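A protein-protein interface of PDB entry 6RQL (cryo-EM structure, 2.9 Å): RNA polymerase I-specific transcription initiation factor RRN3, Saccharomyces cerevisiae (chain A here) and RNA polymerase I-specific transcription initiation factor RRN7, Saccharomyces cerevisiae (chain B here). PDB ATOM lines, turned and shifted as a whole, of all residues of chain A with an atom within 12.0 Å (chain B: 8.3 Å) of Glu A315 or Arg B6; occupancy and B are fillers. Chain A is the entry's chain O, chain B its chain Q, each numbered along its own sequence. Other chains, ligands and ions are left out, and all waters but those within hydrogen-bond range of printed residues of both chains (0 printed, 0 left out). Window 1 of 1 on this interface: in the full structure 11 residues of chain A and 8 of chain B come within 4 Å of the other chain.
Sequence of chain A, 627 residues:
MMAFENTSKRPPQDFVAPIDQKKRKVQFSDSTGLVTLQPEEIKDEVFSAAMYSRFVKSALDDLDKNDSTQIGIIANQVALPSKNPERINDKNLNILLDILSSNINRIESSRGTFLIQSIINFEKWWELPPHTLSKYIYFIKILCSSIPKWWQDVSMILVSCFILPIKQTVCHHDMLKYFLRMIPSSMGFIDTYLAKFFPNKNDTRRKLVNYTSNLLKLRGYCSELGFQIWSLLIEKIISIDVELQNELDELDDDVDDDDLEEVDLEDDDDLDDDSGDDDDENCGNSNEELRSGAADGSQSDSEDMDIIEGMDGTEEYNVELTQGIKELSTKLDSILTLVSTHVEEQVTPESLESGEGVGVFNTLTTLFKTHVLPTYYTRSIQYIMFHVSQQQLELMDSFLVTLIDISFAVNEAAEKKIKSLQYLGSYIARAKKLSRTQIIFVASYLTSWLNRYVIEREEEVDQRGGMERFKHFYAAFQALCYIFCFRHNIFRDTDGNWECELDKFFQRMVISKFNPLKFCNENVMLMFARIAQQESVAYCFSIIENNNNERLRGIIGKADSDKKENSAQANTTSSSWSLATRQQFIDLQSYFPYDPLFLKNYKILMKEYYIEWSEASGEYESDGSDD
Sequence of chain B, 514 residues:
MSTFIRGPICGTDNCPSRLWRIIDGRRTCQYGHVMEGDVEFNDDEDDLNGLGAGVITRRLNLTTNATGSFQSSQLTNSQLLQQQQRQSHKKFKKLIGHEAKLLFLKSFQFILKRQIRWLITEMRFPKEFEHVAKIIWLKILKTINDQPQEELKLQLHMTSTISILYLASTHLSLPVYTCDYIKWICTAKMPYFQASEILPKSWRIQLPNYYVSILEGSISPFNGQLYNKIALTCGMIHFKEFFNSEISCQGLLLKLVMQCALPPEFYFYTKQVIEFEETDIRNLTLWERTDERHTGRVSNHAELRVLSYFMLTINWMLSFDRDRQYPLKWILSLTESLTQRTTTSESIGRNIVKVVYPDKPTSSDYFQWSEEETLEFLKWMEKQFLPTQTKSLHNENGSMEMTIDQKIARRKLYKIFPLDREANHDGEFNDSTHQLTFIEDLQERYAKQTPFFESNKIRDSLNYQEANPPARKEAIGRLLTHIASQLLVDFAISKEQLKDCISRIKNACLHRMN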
ATOM      1  N   ASP A 306      -1.105  39.274  12.854  1.00  0.00           N
ATOM      2  CA  ASP A 306      -2.471  39.719  13.107  1.00  0.00           C
ATOM      3  C   ASP A 306      -3.276  38.627  13.797  1.00  0.00           C
ATOM      4  O   ASP A 306      -3.866  38.857  14.860  1.00  0.00           O
ATOM      5  CB  ASP A 306      -3.138  40.141  11.799  1.00  0.00           C
ATOM      6  N   ILE A 307      -3.317  37.435  13.181  1.00  0.00           N
ATOM      7  CA  ILE A 307      -3.980  36.227  13.693  1.00  0.00           C
ATOM      8  C   ILE A 307      -5.472  36.456  13.946  1.00  0.00           C
ATOM      9  O   ILE A 307      -6.062  35.902  14.876  1.00  0.00           O
ATOM     10  CB  ILE A 307      -3.279  35.689  14.947  1.00  0.00           C
ATOM     11  N   ILE A 308      -6.085  37.279  13.101  1.00  0.00           N
ATOM     12  CA  ILE A 308      -7.511  37.574  13.173  1.00  0.00           C
ATOM     13  C   ILE A 308      -8.184  36.894  11.984  1.00  0.00           C
ATOM     14  O   ILE A 308      -8.148  37.407  10.857  1.00  0.00           O
ATOM     15  CB  ILE A 308      -7.772  39.089  13.194  1.00  0.00           C
ATOM     16  CG1 ILE A 308      -7.088  39.712  14.415  1.00  0.00           C
ATOM     17  CG2 ILE A 308      -9.266  39.389  13.235  1.00  0.00           C
ATOM     18  CD1 ILE A 308      -7.072  41.227  14.417  1.00  0.00           C
ATOM     19  N   GLU A 309      -8.774  35.725  12.233  1.00  0.00           N
ATOM     20  CA  GLU A 309      -9.421  34.936  11.193  1.00  0.00           C
ATOM     21  C   GLU A 309     -10.802  34.489  11.652  1.00  0.00           C
ATOM     22  O   GLU A 309     -11.299  34.949  12.687  1.00  0.00           O
ATOM     23  CB  GLU A 309      -8.580  33.710  10.830  1.00  0.00           C
ATOM     24  CG  GLU A 309      -7.255  34.002  10.148  1.00  0.00           C
ATOM     25  CD  GLU A 309      -6.476  32.736   9.835  1.00  0.00           C
ATOM     26  OE1 GLU A 309      -6.917  31.645  10.256  1.00  0.00           O
ATOM     27  OE2 GLU A 309      -5.425  32.829   9.169  1.00  0.00           O
ATOM     28  N   GLY A 310     -11.431  33.601  10.886  1.00  0.00           N
ATOM     29  CA  GLY A 310     -12.705  33.029  11.277  1.00  0.00           C
ATOM     30  C   GLY A 310     -12.549  31.715  12.012  1.00  0.00           C
ATOM     31  O   GLY A 310     -12.921  30.658  11.492  1.00  0.00           O
ATOM     32  N   MET A 311     -11.994  31.765  13.220  1.00  0.00           N
ATOM     33  CA  MET A 311     -11.679  30.568  13.996  1.00  0.00           C
ATOM     34  C   MET A 311     -12.536  30.547  15.261  1.00  0.00           C
ATOM     35  O   MET A 311     -12.109  30.963  16.336  1.00  0.00           O
ATOM     36  CB  MET A 311     -10.188  30.526  14.323  1.00  0.00           C
ATOM     37  CG  MET A 311      -9.298  30.361  13.107  1.00  0.00           C
ATOM     38  SD  MET A 311      -9.716  28.849  12.230  1.00  0.00           S
ATOM     39  CE  MET A 311      -9.269  27.618  13.451  1.00  0.00           C
ATOM     40  N   ASP A 312     -13.757  30.021  15.124  1.00  0.00           N
ATOM     41  CA  ASP A 312     -14.661  29.829  16.254  1.00  0.00           C
ATOM     42  C   ASP A 312     -15.364  28.477  16.185  1.00  0.00           C
ATOM     43  O   ASP A 312     -16.474  28.323  16.704  1.00  0.00           O
ATOM     44  CB  ASP A 312     -15.697  30.955  16.341  1.00  0.00           C
ATOM     45  CG  ASP A 312     -15.139  32.219  16.963  1.00  0.00           C
ATOM     46  OD1 ASP A 312     -14.249  32.110  17.828  1.00  0.00           O
ATOM     47  OD2 ASP A 312     -15.600  33.320  16.598  1.00  0.00           O
ATOM     48  N   GLY A 313     -14.731  27.488  15.561  1.00  0.00           N
ATOM     49  CA  GLY A 313     -15.280  26.148  15.531  1.00  0.00           C
ATOM     50  C   GLY A 313     -14.875  25.338  16.744  1.00  0.00           C
ATOM     51  O   GLY A 313     -14.658  25.898  17.823  1.00  0.00           O
ATOM     52  N   THR A 314     -14.759  24.023  16.583  1.00  0.00           N
ATOM     53  CA  THR A 314     -14.320  23.140  17.655  1.00  0.00           C
ATOM     54  C   THR A 314     -12.814  22.956  17.556  1.00  0.00           C
ATOM     55  O   THR A 314     -12.291  22.608  16.492  1.00  0.00           O
ATOM     56  CB  THR A 314     -15.018  21.780  17.600  1.00  0.00           C
ATOM     57  OG1 THR A 314     -14.654  21.106  16.391  1.00  0.00           O
ATOM     58  CG2 THR A 314     -16.528  21.952  17.647  1.00  0.00           C
ATOM     59  N   GLU A 315     -12.127  23.195  18.668  1.00  0.00           N
ATOM     60  CA  GLU A 315     -10.682  23.050  18.810  1.00  0.00           C
ATOM     61  C   GLU A 315     -10.405  22.103  19.960  1.00  0.00           C
ATOM     62  O   GLU A 315      -9.640  22.380  20.887  1.00  0.00           O
ATOM     63  CB  GLU A 315     -10.010  24.406  18.986  1.00  0.00           C
ATOM     64  CG  GLU A 315     -10.117  25.279  17.746  1.00  0.00           C
ATOM     65  CD  GLU A 315      -9.402  26.599  17.892  1.00  0.00           C
ATOM     66  OE1 GLU A 315      -8.901  26.885  18.997  1.00  0.00           O
ATOM     67  OE2 GLU A 315      -9.341  27.354  16.899  1.00  0.00           O
ATOM     68  N   GLU A 316     -11.068  20.953  19.866  1.00  0.00           N
ATOM     69  CA  GLU A 316     -11.343  20.064  20.984  1.00  0.00           C
ATOM     70  C   GLU A 316     -10.089  19.449  21.593  1.00  0.00           C
ATOM     71  O   GLU A 316      -9.076  19.258  20.915  1.00  0.00           O
ATOM     72  CB  GLU A 316     -12.274  18.952  20.497  1.00  0.00           C
ATOM     73  CG  GLU A 316     -11.674  18.109  19.357  1.00  0.00           C
ATOM     74  CD  GLU A 316     -12.606  17.027  18.847  1.00  0.00           C
ATOM     75  OE1 GLU A 316     -13.742  16.925  19.351  1.00  0.00           O
ATOM     76  OE2 GLU A 316     -12.197  16.278  17.940  1.00  0.00           O
ATOM     77  N   TYR A 317     -10.177  19.166  22.897  1.00  0.00           N
ATOM     78  CA  TYR A 317      -9.285  18.275  23.648  1.00  0.00           C
ATOM     79  C   TYR A 317      -7.828  18.745  23.605  1.00  0.00           C
ATOM     80  O   TYR A 317      -6.930  18.099  23.063  1.00  0.00           O
ATOM     81  CB  TYR A 317      -9.447  16.828  23.169  1.00  0.00           C
ATOM     82  CG  TYR A 317     -10.775  16.273  23.615  1.00  0.00           C
ATOM     83  CD1 TYR A 317     -10.966  15.877  24.936  1.00  0.00           C
ATOM     84  CD2 TYR A 317     -11.846  16.176  22.737  1.00  0.00           C
ATOM     85  CE1 TYR A 317     -12.181  15.385  25.367  1.00  0.00           C
ATOM     86  CE2 TYR A 317     -13.068  15.681  23.159  1.00  0.00           C
ATOM     87  CZ  TYR A 317     -13.227  15.291  24.477  1.00  0.00           C
ATOM     88  OH  TYR A 317     -14.432  14.795  24.912  1.00  0.00           O
ATOM     89  N   ASN A 318      -7.631  19.903  24.215  1.00  0.00           N
ATOM     90  CA  ASN A 318      -6.333  20.536  24.363  1.00  0.00           C
ATOM     91  C   ASN A 318      -6.157  20.972  25.813  1.00  0.00           C
ATOM     92  O   ASN A 318      -5.791  22.110  26.117  1.00  0.00           O
ATOM     93  CB  ASN A 318      -6.223  21.704  23.388  1.00  0.00           C
ATOM     94  CG  ASN A 318      -6.323  21.261  21.932  1.00  0.00           C
ATOM     95  OD1 ASN A 318      -5.740  20.256  21.532  1.00  0.00           O
ATOM     96  ND2 ASN A 318      -7.080  22.012  21.139  1.00  0.00           N
ATOM     97  N   VAL A 319      -6.421  20.031  26.727  1.00  0.00           N
ATOM     98  CA  VAL A 319      -6.809  20.372  28.094  1.00  0.00           C
ATOM     99  C   VAL A 319      -5.611  20.845  28.911  1.00  0.00           C
ATOM    100  O   VAL A 319      -5.555  22.015  29.310  1.00  0.00           O
ATOM    101  CB  VAL A 319      -7.507  19.164  28.747  1.00  0.00           C
ATOM    102  CG1 VAL A 319      -7.956  19.503  30.147  1.00  0.00           C
ATOM    103  CG2 VAL A 319      -8.680  18.706  27.900  1.00  0.00           C
ATOM    104  N   GLU A 320      -4.636  19.953  29.139  1.00  0.00           N
ATOM    105  CA  GLU A 320      -3.393  20.139  29.926  1.00  0.00           C
ATOM    106  C   GLU A 320      -3.607  20.906  31.242  1.00  0.00           C
ATOM    107  O   GLU A 320      -3.006  21.947  31.510  1.00  0.00           O
ATOM    108  CB  GLU A 320      -2.259  20.749  29.072  1.00  0.00           C
ATOM    109  CG  GLU A 320      -2.460  22.115  28.380  1.00  0.00           C
ATOM    110  CD  GLU A 320      -1.243  22.554  27.592  1.00  0.00           C
ATOM    111  OE1 GLU A 320      -0.238  21.815  27.583  1.00  0.00           O
ATOM    112  OE2 GLU A 320      -1.293  23.640  26.978  1.00  0.00           O
ATOM    113  N   THR B   3     -14.839  18.156  24.242  1.00  0.00           N
ATOM    114  CA  THR B   3     -15.777  18.881  25.085  1.00  0.00           C
ATOM    115  C   THR B   3     -15.763  20.359  24.745  1.00  0.00           C
ATOM    116  O   THR B   3     -16.814  20.977  24.573  1.00  0.00           O
ATOM    117  CB  THR B   3     -15.446  18.724  26.580  1.00  0.00           C
ATOM    118  OG1 THR B   3     -14.173  19.322  26.860  1.00  0.00           O
ATOM    119  CG2 THR B   3     -15.408  17.257  26.965  1.00  0.00           C
ATOM    120  N   PHE B   4     -14.559  20.914  24.642  1.00  0.00           N
ATOM    121  CA  PHE B   4     -14.399  22.348  24.479  1.00  0.00           C
ATOM    122  C   PHE B   4     -14.725  22.783  23.058  1.00  0.00           C
ATOM    123  O   PHE B   4     -14.404  22.101  22.081  1.00  0.00           O
ATOM    124  CB  PHE B   4     -12.980  22.768  24.843  1.00  0.00           C
ATOM    125  CG  PHE B   4     -12.644  22.526  26.274  1.00  0.00           C
ATOM    126  CD1 PHE B   4     -13.142  23.358  27.255  1.00  0.00           C
ATOM    127  CD2 PHE B   4     -11.831  21.469  26.643  1.00  0.00           C
ATOM    128  CE1 PHE B   4     -12.855  23.139  28.576  1.00  0.00           C
ATOM    129  CE2 PHE B   4     -11.527  21.249  27.973  1.00  0.00           C
ATOM    130  CZ  PHE B   4     -12.039  22.090  28.939  1.00  0.00           C
ATOM    131  N   ILE B   5     -15.395  23.926  22.960  1.00  0.00           N
ATOM    132  CA  ILE B   5     -15.709  24.570  21.694  1.00  0.00           C
ATOM    133  C   ILE B   5     -15.082  25.949  21.754  1.00  0.00           C
ATOM    134  O   ILE B   5     -15.463  26.768  22.600  1.00  0.00           O
ATOM    135  CB  ILE B   5     -17.217  24.665  21.452  1.00  0.00           C
ATOM    136  CG1 ILE B   5     -17.835  23.272  21.388  1.00  0.00           C
ATOM    137  CG2 ILE B   5     -17.486  25.387  20.163  1.00  0.00           C
ATOM    138  CD1 ILE B   5     -19.350  23.273  21.368  1.00  0.00           C
ATOM    139  N   ARG B   6     -14.106  26.203  20.884  1.00  0.00           N
ATOM    140  CA  ARG B   6     -13.403  27.480  20.900  1.00  0.00           C
ATOM    141  C   ARG B   6     -14.323  28.597  20.436  1.00  0.00           C
ATOM    142  O   ARG B   6     -14.870  28.547  19.330  1.00  0.00           O
ATOM    143  CB  ARG B   6     -12.150  27.425  20.029  1.00  0.00           C
ATOM    144  CG  ARG B   6     -11.478  28.798  19.829  1.00  0.00           C
ATOM    145  CD  ARG B   6     -10.957  29.442  21.121  1.00  0.00           C
ATOM    146  NE  ARG B   6      -9.855  28.713  21.739  1.00  0.00           N
ATOM    147  CZ  ARG B   6      -8.576  28.919  21.457  1.00  0.00           C
ATOM    148  NH1 ARG B   6      -7.635  28.211  22.068  1.00  0.00           N
ATOM    149  NH2 ARG B   6      -8.236  29.838  20.567  1.00  0.00           N
ATOM    150  N   GLY B   7     -14.514  29.584  21.303  1.00  0.00           N
ATOM    151  CA  GLY B   7     -15.199  30.798  20.945  1.00  0.00           C
ATOM    152  C   GLY B   7     -14.356  32.005  21.291  1.00  0.00           C
ATOM    153  O   GLY B   7     -13.122  31.964  21.232  1.00  0.00           O
ATOM    154  N   PRO B   8     -15.001  33.097  21.682  1.00  0.00           N
ATOM    155  CA  PRO B   8     -14.252  34.315  22.019  1.00  0.00           C
ATOM    156  C   PRO B   8     -13.475  34.214  23.323  1.00  0.00           C
ATOM    157  O   PRO B   8     -13.575  33.218  24.047  1.00  0.00           O
ATOM    158  CB  PRO B   8     -15.350  35.378  22.126  1.00  0.00           C
ATOM    159  CG  PRO B   8     -16.499  34.820  21.362  1.00  0.00           C
ATOM    160  CD  PRO B   8     -16.443  33.350  21.574  1.00  0.00           C
ATOM    161  N   ILE B   9     -12.698  35.244  23.625  1.00  0.00           N
ATOM    162  CA  ILE B   9     -12.050  35.339  24.923  1.00  0.00           C
ATOM    163  C   ILE B   9     -13.082  35.708  25.981  1.00  0.00           C
ATOM    164  O   ILE B   9     -14.191  36.152  25.674  1.00  0.00           O
ATOM    165  CB  ILE B   9     -10.898  36.351  24.878  1.00  0.00           C
ATOM    166  CG1 ILE B   9     -11.440  37.720  24.469  1.00  0.00           C
ATOM    167  CG2 ILE B   9      -9.833  35.892  23.904  1.00  0.00           C
ATOM    168  CD1 ILE B   9     -10.412  38.810  24.476  1.00  0.00           C
ATOM    169  N   PRO B  16      -8.660  34.267  29.616  1.00  0.00           N
ATOM    170  CA  PRO B  16      -8.631  34.625  28.188  1.00  0.00           C
ATOM    171  C   PRO B  16      -9.039  33.496  27.251  1.00  0.00           C
ATOM    172  O   PRO B  16      -8.763  33.596  26.049  1.00  0.00           O
ATOM    173  CB  PRO B  16      -7.154  34.971  27.982  1.00  0.00           C
ATOM    174  CG  PRO B  16      -6.453  34.062  28.923  1.00  0.00           C
ATOM    175  CD  PRO B  16      -7.324  33.915  30.122  1.00  0.00           C
ATOM    176  N   SER B  17      -9.650  32.445  27.760  1.00  0.00           N
ATOM    177  CA  SER B  17      -9.586  31.144  27.130  1.00  0.00           C
ATOM    178  C   SER B  17     -10.784  30.866  26.231  1.00  0.00           C
ATOM    179  O   SER B  17     -11.593  31.745  25.930  1.00  0.00           O
ATOM    180  CB  SER B  17      -9.475  30.079  28.211  1.00  0.00           C
ATOM    181  OG  SER B  17     -10.698  29.947  28.907  1.00  0.00           O
ATOM    182  N   ARG B  18     -10.878  29.615  25.785  1.00  0.00           N
ATOM    183  CA  ARG B  18     -12.029  29.107  25.062  1.00  0.00           C
ATOM    184  C   ARG B  18     -13.210  28.903  26.005  1.00  0.00           C
ATOM    185  O   ARG B  18     -13.118  29.073  27.223  1.00  0.00           O
ATOM    186  CB  ARG B  18     -11.703  27.778  24.375  1.00  0.00           C
ATOM    187  CG  ARG B  18     -11.584  26.578  25.315  1.00  0.00           C
ATOM    188  CD  ARG B  18     -10.170  26.353  25.820  1.00  0.00           C
ATOM    189  NE  ARG B  18     -10.068  25.119  26.595  1.00  0.00           N
ATOM    190  CZ  ARG B  18      -8.959  24.708  27.203  1.00  0.00           C
ATOM    191  NH1 ARG B  18      -8.964  23.573  27.897  1.00  0.00           N
ATOM    192  NH2 ARG B  18      -7.841  25.408  27.094  1.00  0.00           N
ATOM    193  N   LEU B  19     -14.329  28.499  25.417  1.00  0.00           N
ATOM    194  CA  LEU B  19     -15.577  28.290  26.124  1.00  0.00           C
ATOM    195  C   LEU B  19     -15.888  26.803  26.210  1.00  0.00           C
ATOM    196  O   LEU B  19     -15.230  25.971  25.581  1.00  0.00           O
ATOM    197  CB  LEU B  19     -16.714  29.038  25.427  1.00  0.00           C
ATOM    198  CG  LEU B  19     -16.550  30.546  25.563  1.00  0.00           C
ATOM    199  CD1 LEU B  19     -17.377  31.245  24.531  1.00  0.00           C
ATOM    200  CD2 LEU B  19     -17.004  30.965  26.942  1.00  0.00           C
ATOM    201  N   TRP B  20     -16.904  26.489  27.009  1.00  0.00           N
ATOM    202  CA  TRP B  20     -17.356  25.122  27.215  1.00  0.00           C
ATOM    203  C   TRP B  20     -18.751  25.155  27.805  1.00  0.00           C
ATOM    204  O   TRP B  20     -19.003  25.884  28.764  1.00  0.00           O
ATOM    205  CB  TRP B  20     -16.422  24.355  28.146  1.00  0.00           C
ATOM    206  CG  TRP B  20     -16.881  22.984  28.415  1.00  0.00           C
ATOM    207  CD1 TRP B  20     -17.215  22.053  27.495  1.00  0.00           C
ATOM    208  CD2 TRP B  20     -16.990  22.349  29.690  1.00  0.00           C
ATOM    209  NE1 TRP B  20     -17.567  20.882  28.108  1.00  0.00           N
ATOM    210  CE2 TRP B  20     -17.433  21.034  29.460  1.00  0.00           C
ATOM    211  CE3 TRP B  20     -16.768  22.767  31.004  1.00  0.00           C
ATOM    212  CZ2 TRP B  20     -17.663  20.128  30.494  1.00  0.00           C
ATOM    213  CZ3 TRP B  20     -16.996  21.867  32.034  1.00  0.00           C
ATOM    214  CH2 TRP B  20     -17.438  20.562  31.771  1.00  0.00           C
ATOM    215  N   ARG B  27     -22.852  28.315  28.612  1.00  0.00           N
ATOM    216  CA  ARG B  27     -21.454  28.044  28.324  1.00  0.00           C
ATOM    217  C   ARG B  27     -20.537  28.795  29.276  1.00  0.00           C
ATOM    218  O   ARG B  27     -20.742  29.972  29.573  1.00  0.00           O
ATOM    219  CB  ARG B  27     -21.108  28.367  26.865  1.00  0.00           C
ATOM    220  CG  ARG B  27     -21.246  29.802  26.427  1.00  0.00           C
ATOM    221  CD  ARG B  27     -20.845  29.946  24.977  1.00  0.00           C
ATOM    222  NE  ARG B  27     -20.760  31.346  24.572  1.00  0.00           N
ATOM    223  CZ  ARG B  27     -21.764  32.033  24.057  1.00  0.00           C
ATOM    224  NH1 ARG B  27     -21.599  33.301  23.723  1.00  0.00           N
ATOM    225  NH2 ARG B  27     -22.939  31.448  23.867  1.00  0.00           N
ATOM    226  N   GLN B  30     -13.178  27.347  30.929  1.00  0.00           N
ATOM    227  CA  GLN B  30     -12.724  26.201  31.701  1.00  0.00           C
ATOM    228  C   GLN B  30     -12.230  26.583  33.086  1.00  0.00           C
ATOM    229  O   GLN B  30     -11.996  25.691  33.906  1.00  0.00           O
ATOM    230  CB  GLN B  30     -11.626  25.429  30.976  1.00  0.00           C
ATOM    231  CG  GLN B  30     -10.276  26.082  30.965  1.00  0.00           C
ATOM    232  CD  GLN B  30     -10.032  26.886  29.722  1.00  0.00           C
ATOM    233  OE1 GLN B  30     -10.962  27.268  29.015  1.00  0.00           O
ATOM    234  NE2 GLN B  30      -8.763  27.109  29.420  1.00  0.00           N
ATOM    235  N   ALA B  66     -22.735  25.022  15.800  1.00  0.00           N
ATOM    236  CA  ALA B  66     -22.139  25.710  16.952  1.00  0.00           C
ATOM    237  C   ALA B  66     -23.192  26.116  17.987  1.00  0.00           C
ATOM    238  O   ALA B  66     -23.443  27.301  18.216  1.00  0.00           O
ATOM    239  CB  ALA B  66     -21.285  26.908  16.521  1.00  0.00           C
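OH of Tyr A317 sits close to N of Thr B3, 3.5 Å away.
The backbone carbonyl oxygen of Arg B6 sits close to the backbone carbonyl oxygen of Asp A312, at 3.1 Å.
The backbone NH (N) of Arg B6 sits at hydrogen-bond distance from the backbone carbonyl oxygen (O) of Gly A313, at 3.1 Å.
The side-chain carboxylate of Glu A315 is in salt-bridge range of the guanidinium group of Arg B6, 3.4 Å away.
NH2 of Arg B18 lies close to NE2 of Gln B30 (3.0 Å).
O of Glu A315 lies within hydrogen-bond range of ND2 of Asn A318, at 2.6 Å.
The backbone NH (N) of Ile B5 lies within hydrogen-bond range of the backbone carbonyl oxygen (O) of Leu B19, 3.3 Å away.
The backbone carbonyl oxygen (O) of Glu A316 lies within hydrogen-bond range of the side-chain amide nitrogen (ND2) of Asn A318 (3.4 Å).
Among the printed residues, pairs that only touch across the chains: Asp A312 with Gly B7 (3.5 Å), Gly A313 with Ile B5 (3.7 Å), Val A319 with Phe B4 (3.8 Å), Glu A316 with Phe B4 (3.8 Å), Val A319 with Arg B18 (3.9 Å) and Asn A318 with Arg B18 (3.9 Å).
Glu A315 touches just one residue of chain B: Arg B6.
Of chain A, only Asp A312, Gly A313 and Glu A315 come within 4 Å of Arg B6.
Ile B5 touches just one residue of chain A: Gly A313 (3.7 Å).
Of chain A, only Asp A312 comes within 4 Å of Gly B7.
No residue of chain A comes within 4 Å of Pro B8.
Of chain A, only Asn A318 (3.9 Å) and Val A319 (3.9 Å) come within 4 Å of Arg B18.
Of the printed residues of chain A, Phe B4 touches Glu A316 (3.8 Å) and Val A319 (3.8 Å).
Of the printed residues of chain B, Gly A313 touches Ile B5 and Arg B6.
Of the printed residues of chain B, Tyr A317 touches Thr B3 (3.2 Å).
Printed residues of chain A within 4 Å of Thr B3: Tyr A317 (3.2 Å).
Of the printed residues of chain B, Glu A316 touches Phe B4 (3.8 Å).
The nearest residue of chain A that does not touch Arg B6 is Met A311 (4.2 Å).
Of the 15 printed residues of chain B, 6 touch a printed residue of chain A.
Hydrophobic or aromatic side chains of chain B within 4 Å of the printed part of chain A: Phe B4 and Ile B5.
Of the 15 printed residues of chain A, 7 touch a printed residue of chain B.
Hydrophobic or aromatic side chains of chain A within 4 Å of the printed part of chain B: Tyr A317 and Val A319.
Among the printed residues, 10 pairs touch across the chains.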
